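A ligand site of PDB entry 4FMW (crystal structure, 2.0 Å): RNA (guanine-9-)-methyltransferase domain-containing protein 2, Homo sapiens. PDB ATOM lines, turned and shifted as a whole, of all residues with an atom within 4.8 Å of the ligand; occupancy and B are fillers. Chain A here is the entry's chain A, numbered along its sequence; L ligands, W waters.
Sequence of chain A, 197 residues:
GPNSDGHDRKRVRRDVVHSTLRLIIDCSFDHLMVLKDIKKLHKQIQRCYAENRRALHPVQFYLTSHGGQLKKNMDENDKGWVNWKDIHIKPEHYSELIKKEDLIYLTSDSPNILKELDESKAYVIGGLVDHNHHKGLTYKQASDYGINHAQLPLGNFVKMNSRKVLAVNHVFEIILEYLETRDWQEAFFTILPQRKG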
ATOM      1  N   TYR A 105     -27.163  10.711   3.264  1.00  0.00           N
ATOM      2  CA  TYR A 105     -26.682   9.333   3.300  1.00  0.00           C
ATOM      3  C   TYR A 105     -27.644   8.437   2.541  1.00  0.00           C
ATOM      4  O   TYR A 105     -28.822   8.357   2.898  1.00  0.00           O
ATOM      5  CB  TYR A 105     -26.491   8.831   4.741  1.00  0.00           C
ATOM      6  CG  TYR A 105     -25.357   7.838   4.895  1.00  0.00           C
ATOM      7  CD1 TYR A 105     -24.264   8.123   5.704  1.00  0.00           C
ATOM      8  CD2 TYR A 105     -25.360   6.627   4.191  1.00  0.00           C
ATOM      9  CE1 TYR A 105     -23.206   7.215   5.836  1.00  0.00           C
ATOM     10  CE2 TYR A 105     -24.302   5.732   4.289  1.00  0.00           C
ATOM     11  CZ  TYR A 105     -23.226   6.022   5.115  1.00  0.00           C
ATOM     12  OH  TYR A 105     -22.194   5.136   5.231  1.00  0.00           O
ATOM     13  N   LEU A 106     -27.145   7.774   1.491  1.00  0.00           N
ATOM     14  CA  LEU A 106     -27.978   6.857   0.706  1.00  0.00           C
ATOM     15  C   LEU A 106     -28.085   5.547   1.476  1.00  0.00           C
ATOM     16  O   LEU A 106     -27.055   4.996   1.884  1.00  0.00           O
ATOM     17  CB  LEU A 106     -27.382   6.620  -0.698  1.00  0.00           C
ATOM     18  CG  LEU A 106     -27.286   7.853  -1.627  1.00  0.00           C
ATOM     19  CD1 LEU A 106     -26.355   7.570  -2.778  1.00  0.00           C
ATOM     20  CD2 LEU A 106     -28.656   8.286  -2.146  1.00  0.00           C
ATOM     21  N   THR A 107     -29.313   5.095   1.747  1.00  0.00           N
ATOM     22  CA  THR A 107     -29.585   3.849   2.482  1.00  0.00           C
ATOM     23  C   THR A 107     -30.957   3.297   2.127  1.00  0.00           C
ATOM     24  O   THR A 107     -31.936   4.039   2.116  1.00  0.00           O
ATOM     25  CB  THR A 107     -29.386   4.002   4.025  1.00  0.00           C
ATOM     26  OG1 THR A 107     -29.884   2.840   4.688  1.00  0.00           O
ATOM     27  CG2 THR A 107     -30.044   5.275   4.599  1.00  0.00           C
ATOM     28  N   SER A 108     -31.030   1.977   1.867  1.00  0.00           N
ATOM     29  CA  SER A 108     -32.248   1.245   1.510  1.00  0.00           C
ATOM     30  C   SER A 108     -33.314   1.249   2.628  1.00  0.00           C
ATOM     31  O   SER A 108     -34.497   1.039   2.345  1.00  0.00           O
ATOM     32  CB  SER A 108     -31.906  -0.199   1.158  1.00  0.00           C
ATOM     33  OG  SER A 108     -31.234  -0.836   2.227  1.00  0.00           O
ATOM     34  N   ASP A 109     -32.884   1.474   3.883  1.00  0.00           N
ATOM     35  CA  ASP A 109     -33.741   1.459   5.064  1.00  0.00           C
ATOM     36  C   ASP A 109     -34.342   2.843   5.398  1.00  0.00           C
ATOM     37  O   ASP A 109     -35.196   2.932   6.289  1.00  0.00           O
ATOM     38  CB  ASP A 109     -32.983   0.878   6.262  1.00  0.00           C
ATOM     39  CG  ASP A 109     -32.465  -0.519   5.995  1.00  0.00           C
ATOM     40  OD1 ASP A 109     -33.294  -1.441   5.860  1.00  0.00           O
ATOM     41  OD2 ASP A 109     -31.231  -0.669   5.871  1.00  0.00           O
ATOM     42  N   VAL A 124     -23.676   9.985   0.235  1.00  0.00           N
ATOM     43  CA  VAL A 124     -22.813   8.993   0.860  1.00  0.00           C
ATOM     44  C   VAL A 124     -23.302   7.566   0.625  1.00  0.00           C
ATOM     45  O   VAL A 124     -24.477   7.258   0.834  1.00  0.00           O
ATOM     46  CB  VAL A 124     -22.600   9.260   2.389  1.00  0.00           C
ATOM     47  CG1 VAL A 124     -21.379   8.501   2.909  1.00  0.00           C
ATOM     48  CG2 VAL A 124     -22.464  10.741   2.684  1.00  0.00           C
ATOM     49  N   ILE A 125     -22.364   6.688   0.214  1.00  0.00           N
ATOM     50  CA  ILE A 125     -22.594   5.262   0.021  1.00  0.00           C
ATOM     51  C   ILE A 125     -21.756   4.549   1.094  1.00  0.00           C
ATOM     52  O   ILE A 125     -20.574   4.875   1.256  1.00  0.00           O
ATOM     53  CB  ILE A 125     -22.221   4.771  -1.420  1.00  0.00           C
ATOM     54  CG1 ILE A 125     -22.945   5.601  -2.512  1.00  0.00           C
ATOM     55  CG2 ILE A 125     -22.519   3.254  -1.591  1.00  0.00           C
ATOM     56  CD1 ILE A 125     -22.357   5.437  -3.959  1.00  0.00           C
ATOM     57  N   GLY A 126     -22.374   3.626   1.819  1.00  0.00           N
ATOM     58  CA  GLY A 126     -21.677   2.858   2.846  1.00  0.00           C
ATOM     59  C   GLY A 126     -20.734   1.858   2.222  1.00  0.00           C
ATOM     60  O   GLY A 126     -21.167   1.002   1.448  1.00  0.00           O
ATOM     61  N   LEU A 128     -19.505  -1.010   2.566  1.00  0.00           N
ATOM     62  CA  LEU A 128     -19.794  -2.237   3.284  1.00  0.00           C
ATOM     63  C   LEU A 128     -20.367  -3.329   2.377  1.00  0.00           C
ATOM     64  O   LEU A 128     -21.292  -3.076   1.601  1.00  0.00           O
ATOM     65  CB  LEU A 128     -20.783  -1.911   4.433  1.00  0.00           C
ATOM     66  CG  LEU A 128     -21.213  -3.039   5.395  1.00  0.00           C
ATOM     67  CD1 LEU A 128     -20.085  -3.437   6.340  1.00  0.00           C
ATOM     68  CD2 LEU A 128     -22.420  -2.600   6.226  1.00  0.00           C
ATOM     69  N   ASP A 130     -22.193  -6.162   3.261  1.00  0.00           N
ATOM     70  CA  ASP A 130     -23.027  -6.592   4.380  1.00  0.00           C
ATOM     71  C   ASP A 130     -23.410  -8.078   4.437  1.00  0.00           C
ATOM     72  O   ASP A 130     -23.298  -8.670   5.519  1.00  0.00           O
ATOM     73  CB  ASP A 130     -24.312  -5.737   4.424  1.00  0.00           C
ATOM     74  CG  ASP A 130     -25.185  -6.009   5.634  1.00  0.00           C
ATOM     75  N   HIS A 134     -25.784  -6.622   8.775  1.00  0.00           N
ATOM     76  CA  HIS A 134     -25.914  -5.331   9.460  1.00  0.00           C
ATOM     77  C   HIS A 134     -27.085  -4.536   8.871  1.00  0.00           C
ATOM     78  O   HIS A 134     -26.893  -3.457   8.310  1.00  0.00           O
ATOM     79  CB  HIS A 134     -24.593  -4.549   9.394  1.00  0.00           C
ATOM     80  CG  HIS A 134     -23.448  -5.230  10.072  1.00  0.00           C
ATOM     81  ND1 HIS A 134     -22.502  -5.932   9.349  1.00  0.00           N
ATOM     82  CD2 HIS A 134     -23.150  -5.309  11.382  1.00  0.00           C
ATOM     83  CE1 HIS A 134     -21.645  -6.410  10.243  1.00  0.00           C
ATOM     84  NE2 HIS A 134     -22.000  -6.065  11.482  1.00  0.00           N
ATOM     85  N   LYS A 135     -28.311  -5.090   9.006  1.00  0.00           N
ATOM     86  CA  LYS A 135     -29.539  -4.479   8.492  1.00  0.00           C
ATOM     87  C   LYS A 135     -29.882  -3.200   9.259  1.00  0.00           C
ATOM     88  O   LYS A 135     -29.947  -3.205  10.497  1.00  0.00           O
ATOM     89  CB  LYS A 135     -30.715  -5.482   8.548  1.00  0.00           C
ATOM     90  N   GLY A 136     -30.050  -2.108   8.512  1.00  0.00           N
ATOM     91  CA  GLY A 136     -30.375  -0.792   9.061  1.00  0.00           C
ATOM     92  C   GLY A 136     -29.229  -0.050   9.728  1.00  0.00           C
ATOM     93  O   GLY A 136     -29.476   0.941  10.410  1.00  0.00           O
ATOM     94  N   LEU A 137     -27.974  -0.508   9.512  1.00  0.00           N
ATOM     95  CA  LEU A 137     -26.769   0.083  10.123  1.00  0.00           C
ATOM     96  C   LEU A 137     -26.477   1.519   9.649  1.00  0.00           C
ATOM     97  O   LEU A 137     -26.311   2.396  10.493  1.00  0.00           O
ATOM     98  CB  LEU A 137     -25.537  -0.811   9.901  1.00  0.00           C
ATOM     99  CG  LEU A 137     -24.220  -0.366  10.570  1.00  0.00           C
ATOM    100  CD1 LEU A 137     -24.231  -0.614  12.074  1.00  0.00           C
ATOM    101  CD2 LEU A 137     -23.043  -1.071   9.941  1.00  0.00           C
ATOM    102  N   THR A 138     -26.404   1.756   8.312  1.00  0.00           N
ATOM    103  CA  THR A 138     -26.123   3.093   7.754  1.00  0.00           C
ATOM    104  C   THR A 138     -27.248   4.081   8.061  1.00  0.00           C
ATOM    105  O   THR A 138     -26.966   5.258   8.287  1.00  0.00           O
ATOM    106  CB  THR A 138     -25.822   3.045   6.254  1.00  0.00           C
ATOM    107  OG1 THR A 138     -26.912   2.415   5.570  1.00  0.00           O
ATOM    108  CG2 THR A 138     -24.511   2.345   5.928  1.00  0.00           C
ATOM    109  N   ALA A 150     -31.812   9.104   2.384  1.00  0.00           N
ATOM    110  CA  ALA A 150     -32.790   8.749   1.360  1.00  0.00           C
ATOM    111  C   ALA A 150     -32.479   7.410   0.705  1.00  0.00           C
ATOM    112  O   ALA A 150     -31.309   7.013   0.637  1.00  0.00           O
ATOM    113  CB  ALA A 150     -32.848   9.848   0.290  1.00  0.00           C
ATOM    114  N   GLN A 151     -33.524   6.718   0.216  1.00  0.00           N
ATOM    115  CA  GLN A 151     -33.373   5.465  -0.513  1.00  0.00           C
ATOM    116  C   GLN A 151     -33.589   5.719  -2.002  1.00  0.00           C
ATOM    117  O   GLN A 151     -34.288   6.669  -2.356  1.00  0.00           O
ATOM    118  CB  GLN A 151     -34.325   4.367   0.010  1.00  0.00           C
ATOM    119  CG  GLN A 151     -35.815   4.638  -0.174  1.00  0.00           C
ATOM    120  CD  GLN A 151     -36.637   3.390   0.015  1.00  0.00           C
ATOM    121  OE1 GLN A 151     -36.957   2.680  -0.946  1.00  0.00           O
ATOM    122  NE2 GLN A 151     -36.995   3.087   1.247  1.00  0.00           N
ATOM    123  N   LEU A 152     -32.984   4.880  -2.862  1.00  0.00           N
ATOM    124  CA  LEU A 152     -33.145   4.992  -4.311  1.00  0.00           C
ATOM    125  C   LEU A 152     -34.609   4.665  -4.681  1.00  0.00           C
ATOM    126  O   LEU A 152     -35.203   3.797  -4.025  1.00  0.00           O
ATOM    127  CB  LEU A 152     -32.169   4.063  -5.067  1.00  0.00           C
ATOM    128  CG  LEU A 152     -30.679   4.459  -5.025  1.00  0.00           C
ATOM    129  CD1 LEU A 152     -29.812   3.297  -5.467  1.00  0.00           C
ATOM    130  CD2 LEU A 152     -30.389   5.689  -5.894  1.00  0.00           C
ATOM    131  N   LEU A 154     -36.414   2.640  -6.201  1.00  0.00           N
ATOM    132  CA  LEU A 154     -36.511   1.304  -6.802  1.00  0.00           C
ATOM    133  C   LEU A 154     -37.959   0.832  -7.013  1.00  0.00           C
ATOM    134  O   LEU A 154     -38.203   0.020  -7.905  1.00  0.00           O
ATOM    135  CB  LEU A 154     -35.739   0.262  -5.972  1.00  0.00           C
ATOM    136  CG  LEU A 154     -34.202   0.369  -5.968  1.00  0.00           C
ATOM    137  CD1 LEU A 154     -33.600  -0.513  -4.894  1.00  0.00           C
ATOM    138  CD2 LEU A 154     -33.605   0.013  -7.324  1.00  0.00           C
ATOM    139  N   LYS A 164     -33.877  -5.422  -1.273  1.00  0.00           N
ATOM    140  CA  LYS A 164     -33.729  -4.279  -2.180  1.00  0.00           C
ATOM    141  C   LYS A 164     -32.322  -3.632  -2.010  1.00  0.00           C
ATOM    142  O   LYS A 164     -32.037  -2.600  -2.629  1.00  0.00           O
ATOM    143  CB  LYS A 164     -34.844  -3.244  -1.944  1.00  0.00           C
ATOM    144  CG  LYS A 164     -36.259  -3.780  -2.192  1.00  0.00           C
ATOM    145  CD  LYS A 164     -37.074  -2.883  -3.113  1.00  0.00           C
ATOM    146  CE  LYS A 164     -37.957  -1.918  -2.356  1.00  0.00           C
ATOM    147  NZ  LYS A 164     -38.830  -1.138  -3.268  1.00  0.00           N
ATOM    148  N   VAL A 165     -31.475  -4.268  -1.176  1.00  0.00           N
ATOM    149  CA  VAL A 165     -30.103  -3.858  -0.856  1.00  0.00           C
ATOM    150  C   VAL A 165     -29.202  -4.087  -2.067  1.00  0.00           C
ATOM    151  O   VAL A 165     -29.052  -5.228  -2.528  1.00  0.00           O
ATOM    152  CB  VAL A 165     -29.590  -4.580   0.428  1.00  0.00           C
ATOM    153  CG1 VAL A 165     -28.119  -4.275   0.685  1.00  0.00           C
ATOM    154  CG2 VAL A 165     -30.435  -4.222   1.647  1.00  0.00           C
ATOM    155  N   LEU A 166     -28.609  -3.006  -2.594  1.00  0.00           N
ATOM    156  CA  LEU A 166     -27.735  -3.055  -3.767  1.00  0.00           C
ATOM    157  C   LEU A 166     -26.259  -2.961  -3.394  1.00  0.00           C
ATOM    158  O   LEU A 166     -25.926  -2.430  -2.340  1.00  0.00           O
ATOM    159  CB  LEU A 166     -28.102  -1.929  -4.777  1.00  0.00           C
ATOM    160  CG  LEU A 166     -29.603  -1.672  -5.071  1.00  0.00           C
ATOM    161  CD1 LEU A 166     -29.779  -0.493  -5.981  1.00  0.00           C
ATOM    162  CD2 LEU A 166     -30.289  -2.900  -5.674  1.00  0.00           C
ATOM    163  N   ALA A 167     -25.379  -3.479  -4.279  1.00  0.00           N
ATOM    164  CA  ALA A 167     -23.933  -3.440  -4.096  1.00  0.00           C
ATOM    165  C   ALA A 167     -23.425  -1.998  -4.227  1.00  0.00           C
ATOM    166  O   ALA A 167     -24.080  -1.181  -4.878  1.00  0.00           O
ATOM    167  CB  ALA A 167     -23.244  -4.336  -5.117  1.00  0.00           C
ATOM    168  N   VAL A 168     -22.263  -1.697  -3.592  1.00  0.00           N
ATOM    169  CA  VAL A 168     -21.614  -0.380  -3.591  1.00  0.00           C
ATOM    170  C   VAL A 168     -21.496   0.199  -5.021  1.00  0.00           C
ATOM    171  O   VAL A 168     -21.946   1.330  -5.252  1.00  0.00           O
ATOM    172  CB  VAL A 168     -20.230  -0.440  -2.861  1.00  0.00           C
ATOM    173  CG1 VAL A 168     -19.398   0.820  -3.098  1.00  0.00           C
ATOM    174  CG2 VAL A 168     -20.400  -0.700  -1.371  1.00  0.00           C
ATOM    175  N   VAL A 171     -24.990   1.178  -6.830  1.00  0.00           N
ATOM    176  CA  VAL A 171     -25.520   2.488  -6.393  1.00  0.00           C
ATOM    177  C   VAL A 171     -24.738   3.630  -7.084  1.00  0.00           C
ATOM    178  O   VAL A 171     -25.361   4.540  -7.632  1.00  0.00           O
ATOM    179  CB  VAL A 171     -25.513   2.623  -4.835  1.00  0.00           C
ATOM    180  CG1 VAL A 171     -26.024   4.000  -4.385  1.00  0.00           C
ATOM    181  CG2 VAL A 171     -26.353   1.515  -4.191  1.00  0.00           C
HETATM  182  N1  LIG L   1     -26.983  -3.296   5.531  1.00  0.00           N
HETATM  183  C1  LIG L   1     -26.141  -2.323   4.845  1.00  0.00           C
HETATM  184  C2  LIG L   1     -26.154  -2.471   3.285  1.00  0.00           C
HETATM  185  C3  LIG L   1     -24.762  -2.416   2.658  1.00  0.00           C
HETATM  186  S1  LIG L   1     -25.029  -2.184   0.878  1.00  0.00           S
HETATM  187  C4  LIG L   1     -26.528  -0.878   5.265  1.00  0.00           C
HETATM  188  O1  LIG L   1     -26.566   0.041   4.411  1.00  0.00           O
HETATM  189  O2  LIG L   1     -26.799  -0.732   6.531  1.00  0.00           O
HETATM  190  C5  LIG L   1     -23.794  -0.936   0.434  1.00  0.00           C
HETATM  191  C6  LIG L   1     -24.346   0.481   0.403  1.00  0.00           C
HETATM  192  O3  LIG L   1     -25.117   0.767  -0.780  1.00  0.00           O
HETATM  193  C7  LIG L   1     -25.242   0.897   1.557  1.00  0.00           C
HETATM  194  O4  LIG L   1     -24.499   1.156   2.750  1.00  0.00           O
HETATM  195  C8  LIG L   1     -25.951   2.122   0.999  1.00  0.00           C
HETATM  196  O5  LIG L   1     -25.187   3.320   1.165  1.00  0.00           O
HETATM  197  C9  LIG L   1     -26.089   1.759  -0.488  1.00  0.00           C
HETATM  198  N2  LIG L   1     -27.412   1.252  -0.866  1.00  0.00           N
HETATM  199  C10 LIG L   1     -27.776  -0.052  -1.055  1.00  0.00           C
HETATM  200  N3  LIG L   1     -29.017  -0.212  -1.433  1.00  0.00           N
HETATM  201  C11 LIG L   1     -29.518   1.077  -1.493  1.00  0.00           C
HETATM  202  C12 LIG L   1     -30.782   1.596  -1.835  1.00  0.00           C
HETATM  203  N4  LIG L   1     -31.816   0.841  -2.214  1.00  0.00           N
HETATM  204  N5  LIG L   1     -30.947   2.941  -1.780  1.00  0.00           N
HETATM  205  C13 LIG L   1     -29.910   3.705  -1.407  1.00  0.00           C
HETATM  206  N6  LIG L   1     -28.672   3.331  -1.070  1.00  0.00           N
HETATM  207  C14 LIG L   1     -28.538   1.993  -1.129  1.00  0.00           C
HETATM  208  O   HOH W   1     -28.571   0.260   2.477  1.00  0.00           O
HETATM  209  O   HOH W   2     -34.536   1.677  -2.408  1.00  0.00           O
HETATM  210  O   HOH W   3     -29.095   0.927   6.463  1.00  0.00           O
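Ser 108 touches the ligand. CA of Ile 125 touches O5 of the ligand, 3.4 Å away. O of Leu 128 touches C5 of the ligand, 3.5 Å away. CG of Asp 130 touches N1 of the ligand (3.3 Å). CA of Gln 151 touches N5 of the ligand, 3.7 Å away. Leu 154 touches the ligand. Val 165 touches the ligand. Val 168 touches the ligand (CG2 to C5, 3.9 Å). Val 171 touches the ligand. Hydrophobic or aromatic side chains that line the ligand: Leu 106, Ile 125, Leu 128, Leu 137, Leu 152, Leu 154, Val 165, Leu 166, Val 168 and Val 171. 18 residues have an atom within 4 Å of the ligand: Leu 106, Thr 107, Ser 108, Ile 125, Gly 126, Leu 128, Asp 130, His 134, Leu 137, Thr 138, Gln 151, Leu 152, Leu 154, Lys 164, Val 165, Leu 166, Val 168 and Val 171.
The backbone carbonyl oxygen of Leu 106 is in hydrogen-bond range of an oxygen (O5) of the ligand (2.6 Å). The backbone NH (N) of Thr 138 lies within hydrogen-bond range of an oxygen (O2) of the ligand (3.1 Å). O1 of the ligand sits at hydrogen-bond distance from OG1 of Thr 138 (2.7 Å). N1 of the ligand sits at hydrogen-bond distance from O of His 134, at 2.8 Å. N of Gly 126 is in hydrogen-bond range of O5 of the ligand. A nitrogen (N5) of the ligand sits at hydrogen-bond distance from the backbone NH (N) of Leu 152 (3.0 Å). N of Leu 166 lies within hydrogen-bond range of N3 of the ligand (3.1 Å). The backbone NH (N) of Leu 137 is in hydrogen-bond range of an oxygen (O2) of the ligand. The backbone NH (N) of Thr 107 is in hydrogen-bond range of a nitrogen (N6) of the ligand (3.4 Å). O of Lys 164 is in hydrogen-bond range of N4 of the ligand (3.5 Å).
Water W1 bridges O1 of the ligand and OG of Ser 108. Water W3 lies within hydrogen-bond range of OG1 of Thr 107, OD2 of Asp 109, OG1 of Thr 138 and O2 of the ligand. Water W2 lies within hydrogen-bond range of the backbone carbonyl oxygen (O) of Leu 152 (2.7 Å), a nitrogen (N4) of the ligand (2.9 Å) and the side-chain amide oxygen (OE1) of Gln 151 (3.0 Å).
The backbone NH (N) of Leu 106 sits at hydrogen-bond distance from the backbone carbonyl oxygen (O) of Val 124, 2.8 Å away. The side-chain hydroxyl (OG1) of Thr 138 is in hydrogen-bond range of the side-chain hydroxyl (OG1) of Thr 107, 3.1 Å away. O of Ala 150 is in hydrogen-bond range of N of Thr 107, 3.0 Å away. N of Asp 109 sits close to OG1 of Thr 107 (3.4 Å). The backbone carbonyl oxygen of Ser 108 lies within hydrogen-bond range of the side-chain amide nitrogen of Gln 151, at 3.4 Å.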
